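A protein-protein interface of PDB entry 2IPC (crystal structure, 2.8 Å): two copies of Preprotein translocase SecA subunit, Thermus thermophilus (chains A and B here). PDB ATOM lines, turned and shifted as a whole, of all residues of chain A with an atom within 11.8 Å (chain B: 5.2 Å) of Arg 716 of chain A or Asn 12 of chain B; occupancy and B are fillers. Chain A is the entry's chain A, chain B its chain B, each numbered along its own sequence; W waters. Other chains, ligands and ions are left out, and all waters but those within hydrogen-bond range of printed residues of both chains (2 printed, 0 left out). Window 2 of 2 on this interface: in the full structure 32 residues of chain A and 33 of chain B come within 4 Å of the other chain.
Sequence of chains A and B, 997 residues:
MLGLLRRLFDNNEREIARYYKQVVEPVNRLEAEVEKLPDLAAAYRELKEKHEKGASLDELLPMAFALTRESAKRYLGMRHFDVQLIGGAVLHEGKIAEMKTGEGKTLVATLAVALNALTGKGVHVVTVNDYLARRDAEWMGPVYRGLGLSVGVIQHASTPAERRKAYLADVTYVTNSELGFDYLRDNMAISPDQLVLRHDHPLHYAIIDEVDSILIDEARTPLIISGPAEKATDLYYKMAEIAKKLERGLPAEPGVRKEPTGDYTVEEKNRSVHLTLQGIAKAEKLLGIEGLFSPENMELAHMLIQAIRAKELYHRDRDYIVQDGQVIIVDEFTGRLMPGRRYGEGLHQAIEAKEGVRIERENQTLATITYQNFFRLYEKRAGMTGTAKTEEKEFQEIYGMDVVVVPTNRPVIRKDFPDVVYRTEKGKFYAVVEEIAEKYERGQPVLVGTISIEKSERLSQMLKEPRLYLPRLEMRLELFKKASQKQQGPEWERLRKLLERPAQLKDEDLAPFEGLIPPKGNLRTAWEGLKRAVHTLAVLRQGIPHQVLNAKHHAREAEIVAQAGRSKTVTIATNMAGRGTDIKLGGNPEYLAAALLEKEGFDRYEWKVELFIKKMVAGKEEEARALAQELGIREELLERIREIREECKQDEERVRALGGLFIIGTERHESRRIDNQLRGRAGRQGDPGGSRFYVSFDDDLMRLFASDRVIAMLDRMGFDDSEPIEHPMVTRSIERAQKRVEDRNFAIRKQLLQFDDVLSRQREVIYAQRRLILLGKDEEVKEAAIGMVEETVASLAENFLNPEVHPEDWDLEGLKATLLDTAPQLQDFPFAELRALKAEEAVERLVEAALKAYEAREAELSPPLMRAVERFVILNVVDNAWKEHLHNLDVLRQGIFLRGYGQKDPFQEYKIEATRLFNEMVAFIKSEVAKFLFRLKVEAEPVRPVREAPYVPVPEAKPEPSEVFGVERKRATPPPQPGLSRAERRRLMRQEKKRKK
No position is printed for both chains.
O of Ile 711 of chain A lies within hydrogen-bond range of NH1 of Arg 6 of chain B, at 3.4 Å. The side-chain carboxylate of Asp 715 of chain A is in salt-bridge range of the guanidinium group of Arg 6 of chain B (2.7 Å). The guanidinium group (NH2) of Arg 716 of chain A is in salt-bridge range of the side-chain carboxylate (OD2) of Asp 10 of chain B (2.7 Å). NH1 of Arg 716 of chain A is in salt-bridge range of OE2 of Glu 13 of chain B (3.1 Å).
Water W1 lies within hydrogen-bond range of NZ of Lys 389 of chain B (2.8 Å), O of Arg 709 of chain A (3.1 Å) and O of Asp 708 of chain A (3.2 Å). Water W2 bridges O of Asn 12 of chain B (2.8 Å) and NH1 of Arg 716 of chain A (2.9 Å).
Of the 12 printed residues of chain B, 5 touch a printed residue of chain A. Printed residues of chain B that touch a printed residue of chain A: Arg 6, Asp 10, Asn 12, Glu 13 and Lys 389. Along chain B the printed residues that touch a printed residue of chain A span positions 6 to 389. Of the 23 printed residues of chain A, 5 touch a printed residue of chain B.
CD of Lys 389 of chain B touches CG of Arg 709 of chain A, 3.7 Å away. Ala 712 of chain A touches Arg 6 of chain B. Ala 712 of chain A touches Asp 10 of chain B (CB to OD1, 3.6 Å). CG of Arg 6 of chain B touches CG of Arg 716 of chain A (2.9 Å). NH1 of Arg 716 of chain A touches O of Asn 12 of chain B, 3.9 Å away.
Asp 698 of chain A touches none of the printed residues of chain B. Printed residues of chain B within 4 Å of Ile 711 of chain A: Arg 6. Of the printed residues of chain B, Asp 715 of chain A touches Arg 6 (2.7 Å). Arg 716 of chain A touches just these residues of chain B: Arg 6, Asp 10, Asn 12 and Glu 13. Arg 6 of chain B touches just these residues of chain A: Ile 711, Ala 712, Asp 715 and Arg 716. No residue of chain A comes within 4 Å of Ile 16 of chain B. Printed residues of chain A within 4 Å of Lys 389 of chain B: Arg 709. No residue of chain A comes within 4 Å of Val 404 of chain B. The nearest residue of chain A that does not touch Asn 12 of chain B is Arg 709 of chain A (7.6 Å).
The side-chain amide nitrogen (ND2) of Asn 11 of chain B sits at hydrogen-bond distance from the side-chain amide oxygen (OD1) of Asn 12 of chain B, at 2.7 Å. N of Val 405 of chain B lies close to ND2 of Asn 12 of chain B, 2.8 Å away.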
ATOM      1  N   ARG A 423      24.763  13.122   9.601  1.00  0.00           N
ATOM      2  CA  ARG A 423      23.508  13.786   9.751  1.00  0.00           C
ATOM      3  C   ARG A 423      23.048  14.545   8.505  1.00  0.00           C
ATOM      4  O   ARG A 423      21.893  14.442   8.067  1.00  0.00           O
ATOM      5  CB  ARG A 423      23.616  14.723  10.910  1.00  0.00           C
ATOM      6  CG  ARG A 423      22.394  15.459  11.106  1.00  0.00           C
ATOM      7  CD  ARG A 423      22.774  16.737  11.594  1.00  0.00           C
ATOM      8  NE  ARG A 423      21.569  17.371  11.959  1.00  0.00           N
ATOM      9  CZ  ARG A 423      21.310  18.618  11.687  1.00  0.00           C
ATOM     10  NH1 ARG A 423      22.158  19.430  11.069  1.00  0.00           N
ATOM     11  NH2 ARG A 423      20.141  19.029  11.962  1.00  0.00           N
ATOM     12  N   PHE A 697      20.587  11.398   6.862  1.00  0.00           N
ATOM     13  CA  PHE A 697      19.159  11.414   7.141  1.00  0.00           C
ATOM     14  C   PHE A 697      18.438  12.102   6.002  1.00  0.00           C
ATOM     15  O   PHE A 697      17.223  11.971   5.858  1.00  0.00           O
ATOM     16  CB  PHE A 697      18.877  12.140   8.463  1.00  0.00           C
ATOM     17  CG  PHE A 697      19.577  11.535   9.670  1.00  0.00           C
ATOM     18  CD1 PHE A 697      20.180  10.259   9.607  1.00  0.00           C
ATOM     19  CD2 PHE A 697      19.640  12.246  10.881  1.00  0.00           C
ATOM     20  CE1 PHE A 697      20.845   9.700  10.732  1.00  0.00           C
ATOM     21  CE2 PHE A 697      20.301  11.701  12.025  1.00  0.00           C
ATOM     22  CZ  PHE A 697      20.904  10.426  11.942  1.00  0.00           C
ATOM     23  N   ASP A 698      19.197  12.814   5.176  1.00  0.00           N
ATOM     24  CA  ASP A 698      18.615  13.531   4.064  1.00  0.00           C
ATOM     25  C   ASP A 698      18.573  12.810   2.735  1.00  0.00           C
ATOM     26  O   ASP A 698      17.690  13.062   1.907  1.00  0.00           O
ATOM     27  CB  ASP A 698      19.303  14.878   3.915  1.00  0.00           C
ATOM     28  CG  ASP A 698      18.867  15.846   5.013  1.00  0.00           C
ATOM     29  OD1 ASP A 698      17.636  15.960   5.227  1.00  0.00           O
ATOM     30  OD2 ASP A 698      19.728  16.483   5.674  1.00  0.00           O
ATOM     31  N   SER A 707       9.783   6.244   7.961  1.00  0.00           N
ATOM     32  CA  SER A 707       8.547   6.680   8.619  1.00  0.00           C
ATOM     33  C   SER A 707       8.574   8.157   9.010  1.00  0.00           C
ATOM     34  O   SER A 707       9.614   8.707   9.362  1.00  0.00           O
ATOM     35  CB  SER A 707       8.279   5.800   9.852  1.00  0.00           C
ATOM     36  OG  SER A 707       7.586   6.486  10.880  1.00  0.00           O
ATOM     37  N   ASP A 708       7.415   8.795   8.942  1.00  0.00           N
ATOM     38  CA  ASP A 708       7.285  10.211   9.271  1.00  0.00           C
ATOM     39  C   ASP A 708       7.599  10.438  10.749  1.00  0.00           C
ATOM     40  O   ASP A 708       7.866  11.556  11.178  1.00  0.00           O
ATOM     41  CB  ASP A 708       5.860  10.647   8.972  1.00  0.00           C
ATOM     42  CG  ASP A 708       5.245   9.822   7.882  1.00  0.00           C
ATOM     43  OD1 ASP A 708       5.493  10.146   6.700  1.00  0.00           O
ATOM     44  OD2 ASP A 708       4.547   8.831   8.204  1.00  0.00           O
ATOM     45  N   ARG A 709       7.557   9.360  11.519  1.00  0.00           N
ATOM     46  CA  ARG A 709       7.836   9.411  12.949  1.00  0.00           C
ATOM     47  C   ARG A 709       9.335   9.354  13.176  1.00  0.00           C
ATOM     48  O   ARG A 709       9.864  10.001  14.091  1.00  0.00           O
ATOM     49  CB  ARG A 709       7.176   8.223  13.663  1.00  0.00           C
ATOM     50  CG  ARG A 709       7.712   7.923  15.073  1.00  0.00           C
ATOM     51  CD  ARG A 709       7.883   6.414  15.274  1.00  0.00           C
ATOM     52  NE  ARG A 709       9.261   5.973  15.070  1.00  0.00           N
ATOM     53  CZ  ARG A 709       9.956   5.312  15.989  1.00  0.00           C
ATOM     54  NH1 ARG A 709       9.386   5.025  17.152  1.00  0.00           N
ATOM     55  NH2 ARG A 709      11.216   4.955  15.769  1.00  0.00           N
ATOM     56  N   VAL A 710      10.007   8.555  12.347  1.00  0.00           N
ATOM     57  CA  VAL A 710      11.452   8.368  12.437  1.00  0.00           C
ATOM     58  C   VAL A 710      12.158   9.589  11.889  1.00  0.00           C
ATOM     59  O   VAL A 710      13.082  10.112  12.512  1.00  0.00           O
ATOM     60  CB  VAL A 710      11.919   7.122  11.642  1.00  0.00           C
ATOM     61  CG1 VAL A 710      13.377   6.837  11.953  1.00  0.00           C
ATOM     62  CG2 VAL A 710      11.043   5.906  11.996  1.00  0.00           C
ATOM     63  N   ILE A 711      11.705  10.052  10.728  1.00  0.00           N
ATOM     64  CA  ILE A 711      12.298  11.231  10.111  1.00  0.00           C
ATOM     65  C   ILE A 711      12.123  12.450  11.040  1.00  0.00           C
ATOM     66  O   ILE A 711      12.579  13.550  10.721  1.00  0.00           O
ATOM     67  CB  ILE A 711      11.645  11.589   8.731  1.00  0.00           C
ATOM     68  CG1 ILE A 711      11.396  10.335   7.880  1.00  0.00           C
ATOM     69  CG2 ILE A 711      12.584  12.511   7.952  1.00  0.00           C
ATOM     70  CD1 ILE A 711      10.592  10.596   6.590  1.00  0.00           C
ATOM     71  N   ALA A 712      11.460  12.258  12.179  1.00  0.00           N
ATOM     72  CA  ALA A 712      11.227  13.340  13.132  1.00  0.00           C
ATOM     73  C   ALA A 712      12.000  13.109  14.422  1.00  0.00           C
ATOM     74  O   ALA A 712      12.603  14.019  14.981  1.00  0.00           O
ATOM     75  CB  ALA A 712       9.745  13.451  13.420  1.00  0.00           C
ATOM     76  N   MET A 713      11.963  11.874  14.893  1.00  0.00           N
ATOM     77  CA  MET A 713      12.655  11.487  16.103  1.00  0.00           C
ATOM     78  C   MET A 713      14.149  11.676  15.901  1.00  0.00           C
ATOM     79  O   MET A 713      14.862  12.172  16.770  1.00  0.00           O
ATOM     80  CB  MET A 713      12.359  10.018  16.394  1.00  0.00           C
ATOM     81  CG  MET A 713      11.552   9.771  17.643  1.00  0.00           C
ATOM     82  SD  MET A 713      12.527  10.145  19.160  1.00  0.00           S
ATOM     83  CE  MET A 713      11.441  11.301  20.020  1.00  0.00           C
ATOM     84  N   LEU A 714      14.610  11.262  14.734  1.00  0.00           N
ATOM     85  CA  LEU A 714      16.012  11.357  14.383  1.00  0.00           C
ATOM     86  C   LEU A 714      16.545  12.757  14.556  1.00  0.00           C
ATOM     87  O   LEU A 714      17.571  12.980  15.186  1.00  0.00           O
ATOM     88  CB  LEU A 714      16.194  10.945  12.933  1.00  0.00           C
ATOM     89  CG  LEU A 714      16.367   9.452  12.731  1.00  0.00           C
ATOM     90  CD1 LEU A 714      16.173   9.125  11.264  1.00  0.00           C
ATOM     91  CD2 LEU A 714      17.746   9.031  13.219  1.00  0.00           C
ATOM     92  N   ASP A 715      15.826  13.704  13.985  1.00  0.00           N
ATOM     93  CA  ASP A 715      16.220  15.094  14.020  1.00  0.00           C
ATOM     94  C   ASP A 715      16.286  15.636  15.424  1.00  0.00           C
ATOM     95  O   ASP A 715      17.313  16.197  15.824  1.00  0.00           O
ATOM     96  CB  ASP A 715      15.248  15.859  13.149  1.00  0.00           C
ATOM     97  CG  ASP A 715      15.286  15.360  11.692  1.00  0.00           C
ATOM     98  OD1 ASP A 715      15.455  14.140  11.479  1.00  0.00           O
ATOM     99  OD2 ASP A 715      15.165  16.169  10.749  1.00  0.00           O
ATOM    100  N   ARG A 716      15.192  15.480  16.169  1.00  0.00           N
ATOM    101  CA  ARG A 716      15.164  15.934  17.555  1.00  0.00           C
ATOM    102  C   ARG A 716      16.329  15.366  18.336  1.00  0.00           C
ATOM    103  O   ARG A 716      16.825  15.989  19.281  1.00  0.00           O
ATOM    104  CB  ARG A 716      13.898  15.483  18.268  1.00  0.00           C
ATOM    105  CG  ARG A 716      12.719  16.249  17.907  1.00  0.00           C
ATOM    106  CD  ARG A 716      11.554  15.961  18.785  1.00  0.00           C
ATOM    107  NE  ARG A 716      10.437  15.453  17.988  1.00  0.00           N
ATOM    108  CZ  ARG A 716       9.161  15.727  18.234  1.00  0.00           C
ATOM    109  NH1 ARG A 716       8.852  16.517  19.255  1.00  0.00           N
ATOM    110  NH2 ARG A 716       8.200  15.199  17.478  1.00  0.00           N
ATOM    111  N   MET A 717      16.762  14.167  17.951  1.00  0.00           N
ATOM    112  CA  MET A 717      17.862  13.513  18.654  1.00  0.00           C
ATOM    113  C   MET A 717      19.088  14.412  18.716  1.00  0.00           C
ATOM    114  O   MET A 717      20.018  14.166  19.482  1.00  0.00           O
ATOM    115  CB  MET A 717      18.197  12.162  18.011  1.00  0.00           C
ATOM    116  CG  MET A 717      19.018  11.251  18.928  1.00  0.00           C
ATOM    117  SD  MET A 717      18.686   9.480  18.630  1.00  0.00           S
ATOM    118  CE  MET A 717      16.913   9.399  19.170  1.00  0.00           C
ATOM    119  N   GLY A 718      19.051  15.460  17.899  1.00  0.00           N
ATOM    120  CA  GLY A 718      20.098  16.453  17.854  1.00  0.00           C
ATOM    121  C   GLY A 718      21.495  15.926  17.705  1.00  0.00           C
ATOM    122  O   GLY A 718      22.333  16.147  18.576  1.00  0.00           O
ATOM    123  N   PHE A 719      21.747  15.244  16.592  1.00  0.00           N
ATOM    124  CA  PHE A 719      23.069  14.677  16.329  1.00  0.00           C
ATOM    125  C   PHE A 719      24.137  15.676  15.878  1.00  0.00           C
ATOM    126  O   PHE A 719      23.849  16.676  15.209  1.00  0.00           O
ATOM    127  CB  PHE A 719      22.976  13.550  15.294  1.00  0.00           C
ATOM    128  CG  PHE A 719      22.496  12.253  15.854  1.00  0.00           C
ATOM    129  CD1 PHE A 719      21.286  11.705  15.417  1.00  0.00           C
ATOM    130  CD2 PHE A 719      23.250  11.573  16.831  1.00  0.00           C
ATOM    131  CE1 PHE A 719      20.821  10.486  15.944  1.00  0.00           C
ATOM    132  CE2 PHE A 719      22.801  10.356  17.369  1.00  0.00           C
ATOM    133  CZ  PHE A 719      21.582   9.808  16.927  1.00  0.00           C
ATOM    134  N   ASP A 720      25.382  15.379  16.241  1.00  0.00           N
ATOM    135  CA  ASP A 720      26.503  16.225  15.884  1.00  0.00           C
ATOM    136  C   ASP A 720      26.668  16.275  14.374  1.00  0.00           C
ATOM    137  O   ASP A 720      27.212  15.375  13.741  1.00  0.00           O
ATOM    138  CB  ASP A 720      27.771  15.717  16.567  1.00  0.00           C
ATOM    139  CG  ASP A 720      27.584  15.546  18.087  1.00  0.00           C
ATOM    140  OD1 ASP A 720      27.323  16.557  18.799  1.00  0.00           O
ATOM    141  OD2 ASP A 720      27.688  14.393  18.570  1.00  0.00           O
ATOM    142  N   ASP A 721      26.141  17.354  13.827  1.00  0.00           N
ATOM    143  CA  ASP A 721      26.144  17.685  12.412  1.00  0.00           C
ATOM    144  C   ASP A 721      27.317  17.243  11.530  1.00  0.00           C
ATOM    145  O   ASP A 721      27.124  16.790  10.403  1.00  0.00           O
ATOM    146  CB  ASP A 721      26.007  19.198  12.321  1.00  0.00           C
ATOM    147  CG  ASP A 721      26.771  19.909  13.458  1.00  0.00           C
ATOM    148  OD1 ASP A 721      27.838  19.382  13.883  1.00  0.00           O
ATOM    149  OD2 ASP A 721      26.308  20.985  13.923  1.00  0.00           O
ATOM    150  N   ILE A 725      27.906   9.176  12.921  1.00  0.00           N
ATOM    151  CA  ILE A 725      26.839   8.870  13.847  1.00  0.00           C
ATOM    152  C   ILE A 725      26.782   7.357  14.097  1.00  0.00           C
ATOM    153  O   ILE A 725      26.731   6.565  13.148  1.00  0.00           O
ATOM    154  CB  ILE A 725      25.532   9.387  13.259  1.00  0.00           C
ATOM    155  CG1 ILE A 725      25.659  10.897  13.083  1.00  0.00           C
ATOM    156  CG2 ILE A 725      24.357   8.998  14.111  1.00  0.00           C
ATOM    157  CD1 ILE A 725      24.500  11.523  12.324  1.00  0.00           C
ATOM    158  N   HIS A 727      24.477   5.012  16.508  1.00  0.00           N
ATOM    159  CA  HIS A 727      23.384   4.929  17.459  1.00  0.00           C
ATOM    160  C   HIS A 727      22.403   3.838  17.041  1.00  0.00           C
ATOM    161  O   HIS A 727      22.075   3.698  15.873  1.00  0.00           O
ATOM    162  CB  HIS A 727      22.699   6.281  17.483  1.00  0.00           C
ATOM    163  CG  HIS A 727      21.780   6.490  18.631  1.00  0.00           C
ATOM    164  ND1 HIS A 727      22.137   7.214  19.746  1.00  0.00           N
ATOM    165  CD2 HIS A 727      20.475   6.167  18.796  1.00  0.00           C
ATOM    166  CE1 HIS A 727      21.092   7.345  20.541  1.00  0.00           C
ATOM    167  NE2 HIS A 727      20.072   6.718  19.982  1.00  0.00           N
ATOM    168  N   MET A 729      19.113   3.485  17.461  1.00  0.00           N
ATOM    169  CA  MET A 729      17.911   4.017  16.834  1.00  0.00           C
ATOM    170  C   MET A 729      18.182   4.387  15.392  1.00  0.00           C
ATOM    171  O   MET A 729      17.299   4.295  14.530  1.00  0.00           O
ATOM    172  CB  MET A 729      17.440   5.255  17.577  1.00  0.00           C
ATOM    173  CG  MET A 729      15.957   5.562  17.417  1.00  0.00           C
ATOM    174  SD  MET A 729      15.557   6.896  16.216  1.00  0.00           S
ATOM    175  CE  MET A 729      17.028   7.939  16.338  1.00  0.00           C
ATOM    176  N   VAL A 730      19.411   4.810  15.133  1.00  0.00           N
ATOM    177  CA  VAL A 730      19.795   5.192  13.789  1.00  0.00           C
ATOM    178  C   VAL A 730      19.975   3.980  12.896  1.00  0.00           C
ATOM    179  O   VAL A 730      19.273   3.841  11.890  1.00  0.00           O
ATOM    180  CB  VAL A 730      21.091   5.981  13.803  1.00  0.00           C
ATOM    181  CG1 VAL A 730      21.576   6.224  12.380  1.00  0.00           C
ATOM    182  CG2 VAL A 730      20.865   7.307  14.510  1.00  0.00           C
ATOM    183  N   SER A 733      16.655   2.334  12.260  1.00  0.00           N
ATOM    184  CA  SER A 733      15.840   3.022  11.269  1.00  0.00           C
ATOM    185  C   SER A 733      16.341   2.877   9.839  1.00  0.00           C
ATOM    186  O   SER A 733      15.545   2.759   8.909  1.00  0.00           O
ATOM    187  CB  SER A 733      15.673   4.496  11.640  1.00  0.00           C
ATOM    188  OG  SER A 733      16.914   5.125  11.830  1.00  0.00           O
ATOM    189  N   ARG B   6      10.635  20.072  14.217  1.00  0.00           N
ATOM    190  CA  ARG B   6       9.679  19.134  14.817  1.00  0.00           C
ATOM    191  C   ARG B   6       8.434  19.881  15.226  1.00  0.00           C
ATOM    192  O   ARG B   6       7.304  19.517  14.862  1.00  0.00           O
ATOM    193  CB  ARG B   6      10.261  18.526  16.078  1.00  0.00           C
ATOM    194  CG  ARG B   6      11.682  18.153  15.919  1.00  0.00           C
ATOM    195  CD  ARG B   6      11.801  17.001  15.005  1.00  0.00           C
ATOM    196  NE  ARG B   6      12.509  17.399  13.803  1.00  0.00           N
ATOM    197  CZ  ARG B   6      12.189  16.996  12.576  1.00  0.00           C
ATOM    198  NH1 ARG B   6      11.156  16.172  12.374  1.00  0.00           N
ATOM    199  NH2 ARG B   6      12.907  17.417  11.539  1.00  0.00           N
ATOM    200  N   ASP B  10       5.207  18.016  12.969  1.00  0.00           N
ATOM    201  CA  ASP B  10       4.118  17.151  13.387  1.00  0.00           C
ATOM    202  C   ASP B  10       2.963  17.722  14.193  1.00  0.00           C
ATOM    203  O   ASP B  10       2.816  18.926  14.463  1.00  0.00           O
ATOM    204  CB  ASP B  10       4.603  15.855  14.119  1.00  0.00           C
ATOM    205  CG  ASP B  10       6.102  15.785  14.328  1.00  0.00           C
ATOM    206  OD1 ASP B  10       6.837  15.550  13.347  1.00  0.00           O
ATOM    207  OD2 ASP B  10       6.544  15.961  15.481  1.00  0.00           O
ATOM    208  N   ASN B  11       2.152  16.742  14.549  1.00  0.00           N
ATOM    209  CA  ASN B  11       0.948  16.783  15.339  1.00  0.00           C
ATOM    210  C   ASN B  11       1.496  16.978  16.789  1.00  0.00           C
ATOM    211  O   ASN B  11       1.086  17.903  17.493  1.00  0.00           O
ATOM    212  CB  ASN B  11       0.238  15.419  15.006  1.00  0.00           C
ATOM    213  CG  ASN B  11      -0.445  14.729  16.184  1.00  0.00           C
ATOM    214  OD1 ASN B  11      -1.567  15.073  16.565  1.00  0.00           O
ATOM    215  ND2 ASN B  11       0.221  13.714  16.738  1.00  0.00           N
ATOM    216  N   ASN B  12       2.495  16.169  17.159  1.00  0.00           N
ATOM    217  CA  ASN B  12       3.143  16.172  18.476  1.00  0.00           C
ATOM    218  C   ASN B  12       3.985  17.375  18.827  1.00  0.00           C
ATOM    219  O   ASN B  12       4.986  17.243  19.530  1.00  0.00           O
ATOM    220  CB  ASN B  12       4.056  14.965  18.594  1.00  0.00           C
ATOM    221  CG  ASN B  12       3.345  13.675  18.343  1.00  0.00           C
ATOM    222  OD1 ASN B  12       2.892  13.406  17.233  1.00  0.00           O
ATOM    223  ND2 ASN B  12       3.236  12.858  19.382  1.00  0.00           N
ATOM    224  N   GLU B  13       3.578  18.544  18.370  1.00  0.00           N
ATOM    225  CA  GLU B  13       4.354  19.736  18.637  1.00  0.00           C
ATOM    226  C   GLU B  13       3.466  20.957  18.707  1.00  0.00           C
ATOM    227  O   GLU B  13       3.581  21.790  19.621  1.00  0.00           O
ATOM    228  CB  GLU B  13       5.381  19.862  17.536  1.00  0.00           C
ATOM    229  CG  GLU B  13       6.565  18.956  17.770  1.00  0.00           C
ATOM    230  CD  GLU B  13       7.511  19.546  18.843  1.00  0.00           C
ATOM    231  OE1 GLU B  13       6.987  20.016  19.896  1.00  0.00           O
ATOM    232  OE2 GLU B  13       8.760  19.550  18.618  1.00  0.00           O
ATOM    233  N   ARG B  14       2.598  21.052  17.702  1.00  0.00           N
ATOM    234  CA  ARG B  14       1.605  22.101  17.592  1.00  0.00           C
ATOM    235  C   ARG B  14       0.617  21.718  18.678  1.00  0.00           C
ATOM    236  O   ARG B  14       0.003  22.560  19.324  1.00  0.00           O
ATOM    237  CB  ARG B  14       0.964  22.019  16.215  1.00  0.00           C
ATOM    238  CG  ARG B  14      -0.004  23.105  15.906  1.00  0.00           C
ATOM    239  CD  ARG B  14      -0.298  23.158  14.407  1.00  0.00           C
ATOM    240  NE  ARG B  14      -1.466  23.994  14.138  1.00  0.00           N
ATOM    241  CZ  ARG B  14      -2.720  23.596  14.336  1.00  0.00           C
ATOM    242  NH1 ARG B  14      -2.951  22.367  14.791  1.00  0.00           N
ATOM    243  NH2 ARG B  14      -3.733  24.431  14.110  1.00  0.00           N
ATOM    244  N   GLU B  15       0.495  20.413  18.879  1.00  0.00           N
ATOM    245  CA  GLU B  15      -0.382  19.881  19.900  1.00  0.00           C
ATOM    246  C   GLU B  15       0.149  20.229  21.275  1.00  0.00           C
ATOM    247  O   GLU B  15      -0.585  20.758  22.104  1.00  0.00           O
ATOM    248  CB  GLU B  15      -0.507  18.365  19.766  1.00  0.00           C
ATOM    249  CG  GLU B  15      -1.660  17.929  18.871  1.00  0.00           C
ATOM    250  CD  GLU B  15      -2.916  17.562  19.661  1.00  0.00           C
ATOM    251  OE1 GLU B  15      -2.889  16.542  20.392  1.00  0.00           O
ATOM    252  OE2 GLU B  15      -3.930  18.295  19.551  1.00  0.00           O
ATOM    253  N   ILE B  16       1.422  19.939  21.521  1.00  0.00           N
ATOM    254  CA  ILE B  16       2.000  20.232  22.825  1.00  0.00           C
ATOM    255  C   ILE B  16       1.811  21.690  23.209  1.00  0.00           C
ATOM    256  O   ILE B  16       1.558  22.001  24.377  1.00  0.00           O
ATOM    257  CB  ILE B  16       3.494  19.845  22.867  1.00  0.00           C
ATOM    258  CG1 ILE B  16       3.634  18.513  23.608  1.00  0.00           C
ATOM    259  CG2 ILE B  16       4.330  20.914  23.567  1.00  0.00           C
ATOM    260  CD1 ILE B  16       2.983  17.321  22.897  1.00  0.00           C
ATOM    261  N   LYS B 389       4.600   5.426  20.660  1.00  0.00           N
ATOM    262  CA  LYS B 389       4.395   6.062  19.366  1.00  0.00           C
ATOM    263  C   LYS B 389       4.644   5.080  18.243  1.00  0.00           C
ATOM    264  O   LYS B 389       4.043   5.158  17.172  1.00  0.00           O
ATOM    265  CB  LYS B 389       5.304   7.264  19.176  1.00  0.00           C
ATOM    266  CG  LYS B 389       4.718   8.254  18.157  1.00  0.00           C
ATOM    267  CD  LYS B 389       5.716   9.349  17.802  1.00  0.00           C
ATOM    268  CE  LYS B 389       5.114  10.602  17.140  1.00  0.00           C
ATOM    269  NZ  LYS B 389       6.069  11.671  16.713  1.00  0.00           N
ATOM    270  N   VAL B 403      -1.698   8.660  19.963  1.00  0.00           N
ATOM    271  CA  VAL B 403      -0.532   8.687  20.836  1.00  0.00           C
ATOM    272  C   VAL B 403       0.030  10.078  20.843  1.00  0.00           C
ATOM    273  O   VAL B 403       0.228  10.678  19.787  1.00  0.00           O
ATOM    274  CB  VAL B 403       0.605   7.747  20.373  1.00  0.00           C
ATOM    275  CG1 VAL B 403       1.800   7.884  21.304  1.00  0.00           C
ATOM    276  CG2 VAL B 403       0.148   6.318  20.366  1.00  0.00           C
ATOM    277  N   VAL B 404       0.283  10.595  22.040  1.00  0.00           N
ATOM    278  CA  VAL B 404       0.861  11.929  22.191  1.00  0.00           C
ATOM    279  C   VAL B 404       2.245  11.806  22.828  1.00  0.00           C
ATOM    280  O   VAL B 404       2.388  11.259  23.926  1.00  0.00           O
ATOM    281  CB  VAL B 404       0.008  12.835  23.088  1.00  0.00           C
ATOM    282  CG1 VAL B 404       0.655  14.196  23.178  1.00  0.00           C
ATOM    283  CG2 VAL B 404      -1.400  12.974  22.532  1.00  0.00           C
ATOM    284  N   VAL B 405       3.257  12.317  22.139  1.00  0.00           N
ATOM    285  CA  VAL B 405       4.605  12.244  22.660  1.00  0.00           C
ATOM    286  C   VAL B 405       4.812  13.447  23.556  1.00  0.00           C
ATOM    287  O   VAL B 405       5.091  14.552  23.089  1.00  0.00           O
ATOM    288  CB  VAL B 405       5.620  12.248  21.518  1.00  0.00           C
ATOM    289  CG1 VAL B 405       7.021  12.039  22.056  1.00  0.00           C
ATOM    290  CG2 VAL B 405       5.252  11.176  20.527  1.00  0.00           C
HETATM  291  O   HOH W   1       7.427  11.911  14.294  1.00  0.00           O
HETATM  292  O   HOH W   2       6.503  14.919  19.854  1.00  0.00           O
